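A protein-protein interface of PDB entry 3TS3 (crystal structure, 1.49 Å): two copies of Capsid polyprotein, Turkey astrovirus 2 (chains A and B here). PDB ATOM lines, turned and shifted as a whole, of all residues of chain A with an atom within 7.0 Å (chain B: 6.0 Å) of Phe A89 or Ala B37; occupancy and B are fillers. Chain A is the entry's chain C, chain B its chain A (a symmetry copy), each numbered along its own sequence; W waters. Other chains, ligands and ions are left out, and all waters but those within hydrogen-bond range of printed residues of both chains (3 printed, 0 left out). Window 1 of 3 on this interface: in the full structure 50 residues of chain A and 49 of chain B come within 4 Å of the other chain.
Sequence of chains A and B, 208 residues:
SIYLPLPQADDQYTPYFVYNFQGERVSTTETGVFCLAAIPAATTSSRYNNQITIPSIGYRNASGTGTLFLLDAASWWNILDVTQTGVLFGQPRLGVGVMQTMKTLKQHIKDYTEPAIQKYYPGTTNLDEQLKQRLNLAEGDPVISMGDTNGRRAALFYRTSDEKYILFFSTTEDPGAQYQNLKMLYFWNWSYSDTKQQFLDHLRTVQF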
ATOM      1  N   VAL A  18      -9.371  22.365  20.172  1.00  0.00           N
ATOM      2  CA  VAL A  18      -9.188  21.452  19.052  1.00  0.00           C
ATOM      3  C   VAL A  18      -9.693  22.168  17.808  1.00  0.00           C
ATOM      4  O   VAL A  18     -10.770  22.730  17.824  1.00  0.00           O
ATOM      5  CB  VAL A  18      -9.979  20.145  19.226  1.00  0.00           C
ATOM      6  CG1 VAL A  18      -9.686  19.175  18.067  1.00  0.00           C
ATOM      7  CG2 VAL A  18      -9.679  19.514  20.569  1.00  0.00           C
ATOM      8  N   GLY A  32     -12.477  11.123  22.263  1.00  0.00           N
ATOM      9  CA  GLY A  32     -11.450  10.958  21.250  1.00  0.00           C
ATOM     10  C   GLY A  32     -11.150  12.101  20.306  1.00  0.00           C
ATOM     11  O   GLY A  32     -10.585  11.873  19.251  1.00  0.00           O
ATOM     12  N   VAL A  33     -11.505  13.321  20.696  1.00  0.00           N
ATOM     13  CA  VAL A  33     -11.208  14.486  19.797  1.00  0.00           C
ATOM     14  C   VAL A  33      -9.799  15.070  20.056  1.00  0.00           C
ATOM     15  O   VAL A  33      -9.245  15.661  19.143  1.00  0.00           O
ATOM     16  CB  VAL A  33     -12.258  15.597  20.045  1.00  0.00           C
ATOM     17  CG1 VAL A  33     -11.943  16.814  19.227  1.00  0.00           C
ATOM     18  CG2 VAL A  33     -13.663  15.089  19.710  1.00  0.00           C
ATOM     19  N   PHE A  34      -9.200  14.711  21.185  1.00  0.00           N
ATOM     20  CA  PHE A  34      -7.778  14.996  21.379  1.00  0.00           C
ATOM     21  C   PHE A  34      -7.036  13.897  22.136  1.00  0.00           C
ATOM     22  O   PHE A  34      -7.601  13.198  22.963  1.00  0.00           O
ATOM     23  CB  PHE A  34      -7.507  16.372  21.971  1.00  0.00           C
ATOM     24  CG  PHE A  34      -8.112  16.589  23.327  1.00  0.00           C
ATOM     25  CD1 PHE A  34      -7.386  16.342  24.479  1.00  0.00           C
ATOM     26  CD2 PHE A  34      -9.384  17.094  23.448  1.00  0.00           C
ATOM     27  CE1 PHE A  34      -7.937  16.568  25.716  1.00  0.00           C
ATOM     28  CE2 PHE A  34      -9.930  17.319  24.687  1.00  0.00           C
ATOM     29  CZ  PHE A  34      -9.207  17.058  25.815  1.00  0.00           C
ATOM     30  N   CYS A  35      -5.754  13.774  21.830  1.00  0.00           N
ATOM     31  CA  CYS A  35      -4.891  12.779  22.417  1.00  0.00           C
ATOM     32  C   CYS A  35      -3.688  13.441  23.076  1.00  0.00           C
ATOM     33  O   CYS A  35      -3.016  14.247  22.455  1.00  0.00           O
ATOM     34  CB  CYS A  35      -4.416  11.835  21.311  1.00  0.00           C
ATOM     35  SG  CYS A  35      -3.046  10.747  21.758  1.00  0.00           S
ATOM     36  N   LEU A  36      -3.414  13.063  24.319  1.00  0.00           N
ATOM     37  CA  LEU A  36      -2.237  13.552  25.017  1.00  0.00           C
ATOM     38  C   LEU A  36      -1.086  12.582  24.808  1.00  0.00           C
ATOM     39  O   LEU A  36      -1.165  11.425  25.187  1.00  0.00           O
ATOM     40  CB  LEU A  36      -2.504  13.685  26.520  1.00  0.00           C
ATOM     41  CG  LEU A  36      -1.286  14.004  27.396  1.00  0.00           C
ATOM     42  CD1 LEU A  36      -0.774  15.419  27.142  1.00  0.00           C
ATOM     43  CD2 LEU A  36      -1.619  13.804  28.870  1.00  0.00           C
ATOM     44  N   ALA A  37      -0.011  13.080  24.206  1.00  0.00           N
ATOM     45  CA  ALA A  37       1.213  12.312  24.015  1.00  0.00           C
ATOM     46  C   ALA A  37       2.312  13.038  24.781  1.00  0.00           C
ATOM     47  O   ALA A  37       2.407  14.245  24.725  1.00  0.00           O
ATOM     48  CB  ALA A  37       1.564  12.200  22.533  1.00  0.00           C
ATOM     49  N   ALA A  38       3.092  12.300  25.551  1.00  0.00           N
ATOM     50  CA  ALA A  38       4.128  12.923  26.356  1.00  0.00           C
ATOM     51  C   ALA A  38       5.191  11.930  26.805  1.00  0.00           C
ATOM     52  O   ALA A  38       4.950  10.731  26.841  1.00  0.00           O
ATOM     53  CB  ALA A  38       3.508  13.612  27.555  1.00  0.00           C
ATOM     54  N   VAL A  87       2.129  17.125  24.261  1.00  0.00           N
ATOM     55  CA  VAL A  87       1.511  17.685  23.067  1.00  0.00           C
ATOM     56  C   VAL A  87       0.129  17.075  22.907  1.00  0.00           C
ATOM     57  O   VAL A  87      -0.137  16.014  23.449  1.00  0.00           O
ATOM     58  CB  VAL A  87       2.330  17.398  21.788  1.00  0.00           C
ATOM     59  CG1 VAL A  87       3.709  18.032  21.871  1.00  0.00           C
ATOM     60  CG2 VAL A  87       2.425  15.901  21.529  1.00  0.00           C
ATOM     61  N   LEU A  88      -0.746  17.750  22.173  1.00  0.00           N
ATOM     62  CA  LEU A  88      -2.035  17.162  21.846  1.00  0.00           C
ATOM     63  C   LEU A  88      -2.114  16.876  20.360  1.00  0.00           C
ATOM     64  O   LEU A  88      -1.856  17.755  19.555  1.00  0.00           O
ATOM     65  CB  LEU A  88      -3.199  18.086  22.212  1.00  0.00           C
ATOM     66  CG  LEU A  88      -3.464  18.475  23.664  1.00  0.00           C
ATOM     67  CD1 LEU A  88      -4.821  19.178  23.767  1.00  0.00           C
ATOM     68  CD2 LEU A  88      -3.421  17.252  24.581  1.00  0.00           C
ATOM     69  N   PHE A  89      -2.471  15.640  20.028  1.00  0.00           N
ATOM     70  CA  PHE A  89      -2.777  15.256  18.658  1.00  0.00           C
ATOM     71  C   PHE A  89      -4.272  15.437  18.486  1.00  0.00           C
ATOM     72  O   PHE A  89      -5.036  15.166  19.391  1.00  0.00           O
ATOM     73  CB  PHE A  89      -2.473  13.780  18.385  1.00  0.00           C
ATOM     74  CG  PHE A  89      -1.020  13.467  18.142  1.00  0.00           C
ATOM     75  CD1 PHE A  89      -0.169  13.244  19.196  1.00  0.00           C
ATOM     76  CD2 PHE A  89      -0.526  13.351  16.859  1.00  0.00           C
ATOM     77  CE1 PHE A  89       1.145  12.936  18.986  1.00  0.00           C
ATOM     78  CE2 PHE A  89       0.795  13.052  16.636  1.00  0.00           C
ATOM     79  CZ  PHE A  89       1.632  12.832  17.699  1.00  0.00           C
ATOM     80  N   GLY A  90      -4.670  15.889  17.310  1.00  0.00           N
ATOM     81  CA  GLY A  90      -6.068  16.033  16.965  1.00  0.00           C
ATOM     82  C   GLY A  90      -6.743  14.734  16.573  1.00  0.00           C
ATOM     83  O   GLY A  90      -6.090  13.771  16.220  1.00  0.00           O
ATOM     84  N   GLN A  91      -8.069  14.763  16.565  1.00  0.00           N
ATOM     85  CA  GLN A  91      -8.898  13.619  16.240  1.00  0.00           C
ATOM     86  C   GLN A  91      -8.412  13.115  14.885  1.00  0.00           C
ATOM     87  O   GLN A  91      -8.129  13.901  14.011  1.00  0.00           O
ATOM     88  CB  GLN A  91     -10.338  14.134  16.114  1.00  0.00           C
ATOM     89  CG  GLN A  91     -11.399  13.086  15.832  1.00  0.00           C
ATOM     90  CD  GLN A  91     -12.754  13.704  15.554  1.00  0.00           C
ATOM     91  OE1 GLN A  91     -12.847  14.843  15.123  1.00  0.00           O
ATOM     92  NE2 GLN A  91     -13.803  12.944  15.796  1.00  0.00           N
ATOM     93  N   PRO A  92      -8.334  11.799  14.710  1.00  0.00           N
ATOM     94  CA  PRO A  92      -7.667  11.248  13.531  1.00  0.00           C
ATOM     95  C   PRO A  92      -8.257  11.712  12.201  1.00  0.00           C
ATOM     96  O   PRO A  92      -7.494  11.959  11.287  1.00  0.00           O
ATOM     97  CB  PRO A  92      -7.834   9.735  13.717  1.00  0.00           C
ATOM     98  CG  PRO A  92      -7.802   9.561  15.196  1.00  0.00           C
ATOM     99  CD  PRO A  92      -8.465  10.789  15.777  1.00  0.00           C
ATOM    100  N   VAL A  96      -4.711  16.744  11.389  1.00  0.00           N
ATOM    101  CA  VAL A  96      -3.909  17.840  11.933  1.00  0.00           C
ATOM    102  C   VAL A  96      -2.659  17.444  12.710  1.00  0.00           C
ATOM    103  O   VAL A  96      -1.765  18.253  12.877  1.00  0.00           O
ATOM    104  CB  VAL A  96      -4.740  18.860  12.759  1.00  0.00           C
ATOM    105  CG1 VAL A  96      -5.747  19.570  11.862  1.00  0.00           C
ATOM    106  CG2 VAL A  96      -5.426  18.184  13.927  1.00  0.00           C
ATOM    107  N   GLY A  97      -2.619  16.216  13.212  1.00  0.00           N
ATOM    108  CA  GLY A  97      -1.493  15.785  14.018  1.00  0.00           C
ATOM    109  C   GLY A  97      -1.325  16.630  15.267  1.00  0.00           C
ATOM    110  O   GLY A  97      -2.302  16.938  15.925  1.00  0.00           O
ATOM    111  N   VAL A  98      -0.099  17.042  15.570  1.00  0.00           N
ATOM    112  CA  VAL A  98       0.118  17.821  16.779  1.00  0.00           C
ATOM    113  C   VAL A  98      -0.411  19.233  16.561  1.00  0.00           C
ATOM    114  O   VAL A  98       0.041  19.941  15.686  1.00  0.00           O
ATOM    115  CB  VAL A  98       1.613  17.887  17.131  1.00  0.00           C
ATOM    116  CG1 VAL A  98       1.875  18.941  18.207  1.00  0.00           C
ATOM    117  CG2 VAL A  98       2.127  16.506  17.557  1.00  0.00           C
ATOM    118  N   MET A  99      -1.408  19.608  17.348  1.00  0.00           N
ATOM    119  CA  MET A  99      -2.041  20.865  17.070  1.00  0.00           C
ATOM    120  C   MET A  99      -2.041  21.727  18.315  1.00  0.00           C
ATOM    121  O   MET A  99      -2.333  22.905  18.181  1.00  0.00           O
ATOM    122  CB  MET A  99      -3.448  20.712  16.442  1.00  0.00           C
ATOM    123  CG  MET A  99      -4.423  19.799  17.192  1.00  0.00           C
ATOM    124  SD  MET A  99      -5.329  20.699  18.469  1.00  0.00           S
ATOM    125  CE  MET A  99      -5.764  19.392  19.614  1.00  0.00           C
ATOM    126  N   GLN A 100      -1.517  21.209  19.419  1.00  0.00           N
ATOM    127  CA  GLN A 100      -1.158  22.026  20.575  1.00  0.00           C
ATOM    128  C   GLN A 100       0.079  21.484  21.241  1.00  0.00           C
ATOM    129  O   GLN A 100       0.332  20.300  21.221  1.00  0.00           O
ATOM    130  CB  GLN A 100      -2.245  22.063  21.664  1.00  0.00           C
ATOM    131  CG  GLN A 100      -3.640  22.389  21.211  1.00  0.00           C
ATOM    132  CD  GLN A 100      -3.899  23.873  21.054  1.00  0.00           C
ATOM    133  OE1 GLN A 100      -3.039  24.711  21.303  1.00  0.00           O
ATOM    134  NE2 GLN A 100      -5.108  24.197  20.644  1.00  0.00           N
ATOM    135  N   TYR A 186      -0.980   6.101  25.450  1.00  0.00           N
ATOM    136  CA  TYR A 186      -1.617   7.320  24.992  1.00  0.00           C
ATOM    137  C   TYR A 186      -2.858   7.538  25.844  1.00  0.00           C
ATOM    138  O   TYR A 186      -3.486   6.589  26.273  1.00  0.00           O
ATOM    139  CB  TYR A 186      -2.077   7.194  23.537  1.00  0.00           C
ATOM    140  CG  TYR A 186      -1.011   7.304  22.467  1.00  0.00           C
ATOM    141  CD1 TYR A 186      -0.457   8.522  22.122  1.00  0.00           C
ATOM    142  CD2 TYR A 186      -0.603   6.188  21.772  1.00  0.00           C
ATOM    143  CE1 TYR A 186       0.494   8.606  21.122  1.00  0.00           C
ATOM    144  CE2 TYR A 186       0.339   6.263  20.787  1.00  0.00           C
ATOM    145  CZ  TYR A 186       0.878   7.468  20.456  1.00  0.00           C
ATOM    146  OH  TYR A 186       1.815   7.512  19.457  1.00  0.00           O
ATOM    147  N   TRP A 188      -6.588   9.679  25.800  1.00  0.00           N
ATOM    148  CA  TRP A 188      -7.536  10.368  24.939  1.00  0.00           C
ATOM    149  C   TRP A 188      -8.691  10.930  25.773  1.00  0.00           C
ATOM    150  O   TRP A 188      -9.046  10.365  26.793  1.00  0.00           O
ATOM    151  CB  TRP A 188      -8.088   9.397  23.894  1.00  0.00           C
ATOM    152  CG  TRP A 188      -7.107   8.945  22.844  1.00  0.00           C
ATOM    153  CD1 TRP A 188      -6.186   7.945  22.957  1.00  0.00           C
ATOM    154  CD2 TRP A 188      -6.990   9.450  21.514  1.00  0.00           C
ATOM    155  NE1 TRP A 188      -5.493   7.810  21.782  1.00  0.00           N
ATOM    156  CE2 TRP A 188      -5.974   8.718  20.879  1.00  0.00           C
ATOM    157  CE3 TRP A 188      -7.648  10.449  20.798  1.00  0.00           C
ATOM    158  CZ2 TRP A 188      -5.594   8.961  19.576  1.00  0.00           C
ATOM    159  CZ3 TRP A 188      -7.275  10.680  19.505  1.00  0.00           C
ATOM    160  CH2 TRP A 188      -6.254   9.944  18.906  1.00  0.00           C
ATOM    161  N   CYS B  35      11.305   7.694  20.531  1.00  0.00           N
ATOM    162  CA  CYS B  35       9.948   7.200  20.538  1.00  0.00           C
ATOM    163  C   CYS B  35       9.175   7.767  19.367  1.00  0.00           C
ATOM    164  O   CYS B  35       9.181   8.967  19.157  1.00  0.00           O
ATOM    165  CB  CYS B  35       9.277   7.643  21.832  1.00  0.00           C
ATOM    166  SG  CYS B  35       7.486   7.400  21.893  1.00  0.00           S
ATOM    167  N   LEU B  36       8.485   6.897  18.639  1.00  0.00           N
ATOM    168  CA  LEU B  36       7.616   7.342  17.569  1.00  0.00           C
ATOM    169  C   LEU B  36       6.192   7.485  18.094  1.00  0.00           C
ATOM    170  O   LEU B  36       5.590   6.521  18.548  1.00  0.00           O
ATOM    171  CB  LEU B  36       7.615   6.326  16.427  1.00  0.00           C
ATOM    172  CG  LEU B  36       6.560   6.546  15.333  1.00  0.00           C
ATOM    173  CD1 LEU B  36       6.885   7.792  14.506  1.00  0.00           C
ATOM    174  CD2 LEU B  36       6.473   5.332  14.444  1.00  0.00           C
ATOM    175  N   ALA B  37       5.665   8.702  18.005  1.00  0.00           N
ATOM    176  CA  ALA B  37       4.292   8.991  18.366  1.00  0.00           C
ATOM    177  C   ALA B  37       3.591   9.447  17.097  1.00  0.00           C
ATOM    178  O   ALA B  37       4.130  10.222  16.347  1.00  0.00           O
ATOM    179  CB  ALA B  37       4.233  10.073  19.430  1.00  0.00           C
ATOM    180  N   ALA B  38       2.421   8.899  16.823  1.00  0.00           N
ATOM    181  CA  ALA B  38       1.710   9.268  15.612  1.00  0.00           C
ATOM    182  C   ALA B  38       0.233   8.960  15.724  1.00  0.00           C
ATOM    183  O   ALA B  38      -0.156   8.090  16.486  1.00  0.00           O
ATOM    184  CB  ALA B  38       2.305   8.538  14.423  1.00  0.00           C
ATOM    185  N   ILE B  39      -0.542   9.580  14.836  1.00  0.00           N
ATOM    186  CA  ILE B  39      -1.842   9.059  14.434  1.00  0.00           C
ATOM    187  C   ILE B  39      -1.484   8.575  13.004  1.00  0.00           C
ATOM    188  O   ILE B  39      -1.366   9.372  12.088  1.00  0.00           O
ATOM    189  CB  ILE B  39      -2.905  10.135  14.294  1.00  0.00           C
ATOM    190  CG1 ILE B  39      -3.077  10.931  15.596  1.00  0.00           C
ATOM    191  CG2 ILE B  39      -4.218   9.514  13.834  1.00  0.00           C
ATOM    192  CD1 ILE B  39      -3.366  10.115  16.772  1.00  0.00           C
ATOM    193  N   THR B  85       1.465  12.721  10.501  1.00  0.00           N
ATOM    194  CA  THR B  85       1.479  13.208  11.874  1.00  0.00           C
ATOM    195  C   THR B  85       2.632  12.733  12.749  1.00  0.00           C
ATOM    196  O   THR B  85       2.770  13.182  13.865  1.00  0.00           O
ATOM    197  CB  THR B  85       0.176  12.822  12.584  1.00  0.00           C
ATOM    198  OG1 THR B  85       0.144  11.407  12.786  1.00  0.00           O
ATOM    199  CG2 THR B  85      -1.032  13.231  11.750  1.00  0.00           C
ATOM    200  N   GLY B  86       3.463  11.841  12.233  1.00  0.00           N
ATOM    201  CA  GLY B  86       4.506  11.255  13.048  1.00  0.00           C
ATOM    202  C   GLY B  86       5.538  12.221  13.589  1.00  0.00           C
ATOM    203  O   GLY B  86       5.946  13.148  12.922  1.00  0.00           O
ATOM    204  N   VAL B  87       5.942  11.978  14.830  1.00  0.00           N
ATOM    205  CA  VAL B  87       7.003  12.746  15.486  1.00  0.00           C
ATOM    206  C   VAL B  87       7.865  11.807  16.310  1.00  0.00           C
ATOM    207  O   VAL B  87       7.418  10.742  16.686  1.00  0.00           O
ATOM    208  CB  VAL B  87       6.465  13.841  16.450  1.00  0.00           C
ATOM    209  CG1 VAL B  87       5.567  14.822  15.720  1.00  0.00           C
ATOM    210  CG2 VAL B  87       5.736  13.222  17.629  1.00  0.00           C
ATOM    211  N   LEU B  88       9.098  12.217  16.585  1.00  0.00           N
ATOM    212  CA  LEU B  88       9.966  11.460  17.476  1.00  0.00           C
ATOM    213  C   LEU B  88      10.228  12.230  18.758  1.00  0.00           C
ATOM    214  O   LEU B  88      10.684  13.359  18.718  1.00  0.00           O
ATOM    215  CB  LEU B  88      11.318  11.173  16.828  1.00  0.00           C
ATOM    216  CG  LEU B  88      11.397  10.306  15.579  1.00  0.00           C
ATOM    217  CD1 LEU B  88      12.838   9.925  15.311  1.00  0.00           C
ATOM    218  CD2 LEU B  88      10.535   9.072  15.725  1.00  0.00           C
ATOM    219  N   PHE B  89       9.953  11.589  19.886  1.00  0.00           N
ATOM    220  CA  PHE B  89      10.325  12.105  21.201  1.00  0.00           C
ATOM    221  C   PHE B  89      11.701  11.545  21.542  1.00  0.00           C
ATOM    222  O   PHE B  89      12.008  10.410  21.218  1.00  0.00           O
ATOM    223  CB  PHE B  89       9.384  11.609  22.299  1.00  0.00           C
ATOM    224  CG  PHE B  89       8.069  12.333  22.390  1.00  0.00           C
ATOM    225  CD1 PHE B  89       7.896  13.381  23.269  1.00  0.00           C
ATOM    226  CD2 PHE B  89       6.988  11.916  21.641  1.00  0.00           C
ATOM    227  CE1 PHE B  89       6.680  14.022  23.377  1.00  0.00           C
ATOM    228  CE2 PHE B  89       5.775  12.552  21.736  1.00  0.00           C
ATOM    229  CZ  PHE B  89       5.616  13.605  22.614  1.00  0.00           C
ATOM    230  N   TYR B 186       2.625   3.459  21.756  1.00  0.00           N
ATOM    231  CA  TYR B 186       3.876   4.125  21.462  1.00  0.00           C
ATOM    232  C   TYR B 186       4.854   3.066  20.965  1.00  0.00           C
ATOM    233  O   TYR B 186       4.787   1.921  21.376  1.00  0.00           O
ATOM    234  CB  TYR B 186       4.479   4.739  22.728  1.00  0.00           C
ATOM    235  CG  TYR B 186       3.874   6.027  23.232  1.00  0.00           C
ATOM    236  CD1 TYR B 186       4.135   7.233  22.613  1.00  0.00           C
ATOM    237  CD2 TYR B 186       3.086   6.037  24.364  1.00  0.00           C
ATOM    238  CE1 TYR B 186       3.615   8.408  23.100  1.00  0.00           C
ATOM    239  CE2 TYR B 186       2.556   7.200  24.848  1.00  0.00           C
ATOM    240  CZ  TYR B 186       2.824   8.381  24.220  1.00  0.00           C
ATOM    241  OH  TYR B 186       2.294   9.534  24.726  1.00  0.00           O
ATOM    242  N   PHE B 187       5.769   3.474  20.098  1.00  0.00           N
ATOM    243  CA  PHE B 187       6.831   2.603  19.621  1.00  0.00           C
ATOM    244  C   PHE B 187       8.169   3.222  19.980  1.00  0.00           C
ATOM    245  O   PHE B 187       8.341   4.418  19.839  1.00  0.00           O
ATOM    246  CB  PHE B 187       6.735   2.390  18.112  1.00  0.00           C
ATOM    247  CG  PHE B 187       5.657   1.432  17.706  1.00  0.00           C
ATOM    248  CD1 PHE B 187       4.349   1.849  17.591  1.00  0.00           C
ATOM    249  CD2 PHE B 187       5.953   0.115  17.439  1.00  0.00           C
ATOM    250  CE1 PHE B 187       3.367   0.964  17.231  1.00  0.00           C
ATOM    251  CE2 PHE B 187       4.969  -0.763  17.078  1.00  0.00           C
ATOM    252  CZ  PHE B 187       3.680  -0.336  16.970  1.00  0.00           C
HETATM  253  O   HOH W   1       3.017   5.402  18.286  1.00  0.00           O
HETATM  254  O   HOH W   2       2.086  15.938  13.920  1.00  0.00           O
HETATM  255  O   HOH W   3       0.454   9.675  26.728  1.00  0.00           O
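The backbone carbonyl oxygen of Ala A37 lies within hydrogen-bond range of the backbone NH of Val A87.
The backbone carbonyl oxygen (O) of Ala B37 is in hydrogen-bond range of the backbone NH (N) of Val B87, at 2.9 Å.
The backbone carbonyl oxygen (O) of Cys B35 is in hydrogen-bond range of the backbone NH (N) of Phe B89 (2.8 Å).
O of Gly A97 sits at hydrogen-bond distance from N of Gly A90 (2.9 Å).
OG1 of Thr B85 is in hydrogen-bond range of O of Ile B39, 2.6 Å away.
The backbone carbonyl oxygen (O) of Cys A35 is in hydrogen-bond range of the backbone NH (N) of Phe A89.
Of the 21 printed residues of chain A, 8 touch a printed residue of chain B.
Hydrophobic or aromatic side chains of chain A within 4 Å of the printed part of chain B: Ala A37, Phe A89, Pro A92, Tyr A186 and Trp A188.
Printed residues of chain B that touch a printed residue of chain A: Ala B37, Ala B38, Ile B39, Thr B85, Phe B89 and Tyr B186.
Along chain B the printed residues that touch a printed residue of chain A span positions 37 to 186.
Printed residues of chain B within 4 Å of Phe A89: Ala B37, Ile B39 and Thr B85.
Of chain A, only Phe A89 and Tyr A186 come within 4 Å of Ala B37.
Of the printed residues of chain A, Ala B38 touches Tyr A186 (3.0 Å).
Printed residues of chain B within 4 Å of Ala A37: Phe B89 (3.9 Å) and Tyr B186 (3.1 Å).
Printed residues of chain A within 4 Å of Phe B89: Ala A37.
Of the printed residues of chain A, Tyr B186 touches Leu A36, Ala A37, Ala A38 and Tyr A186.
Met A99 touches none of the printed residues of chain B.
Leu A88 touches none of the printed residues of chain B.
Leu A36 touches Tyr B186, but with the chains exchanged Tyr A186 does not touch Leu B36 (4.01 Å).
Ala A37 touches Tyr B186, and with the chains exchanged Tyr A186 touches Ala B37.
Ala A38 touches Tyr B186, and with the chains exchanged Tyr A186 touches Ala B38.
Tyr A186 touches its own counterpart, Tyr B186.
Of the 13 pairs that touch across the chains among the printed residues, 7 have their exchanged pair printed and touching as well.
Tyr B186 touches Leu A36.
CZ of Phe B89 touches O of Ala A37, 3.9 Å away.
Ala A37 touches Tyr B186 (CA to OH, 3.1 Å).
Phe A89 touches Ala B37.
CG1 of Ile B39 touches CD2 of Phe A89, at 3.7 Å.
Phe A89 touches Thr B85 (CE2 to O, 3.4 Å).
Pro A92 touches Ile B39 (CB to CG2, 3.6 Å).
Gly A97 touches Thr B85 (CA to CG2, 3.4 Å).
Tyr A186 touches Tyr B186 (CE1 to CE1, 3.7 Å).
Trp A188 touches Ile B39.
The side-chain hydroxyl (OH) of Tyr B186 is in hydrogen-bond range of the backbone NH (N) of Ala A38, at 3.0 Å.
The side-chain hydroxyl (OH) of Tyr A186 lies within hydrogen-bond range of the backbone NH (N) of Ala B38, at 3.0 Å.
Water W1 bridges the side-chain hydroxyl (OH) of Tyr A186 (2.7 Å) and the backbone carbonyl oxygen (O) of Leu B36 (2.8 Å).
Water W3 lies within hydrogen-bond range of OH of Tyr B186 (2.7 Å) and O of Leu A36 (2.8 Å).
Water W2 lies within hydrogen-bond range of the backbone carbonyl oxygen of Thr B85 (2.8 Å) and the backbone NH of Val A98 (3.0 Å).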
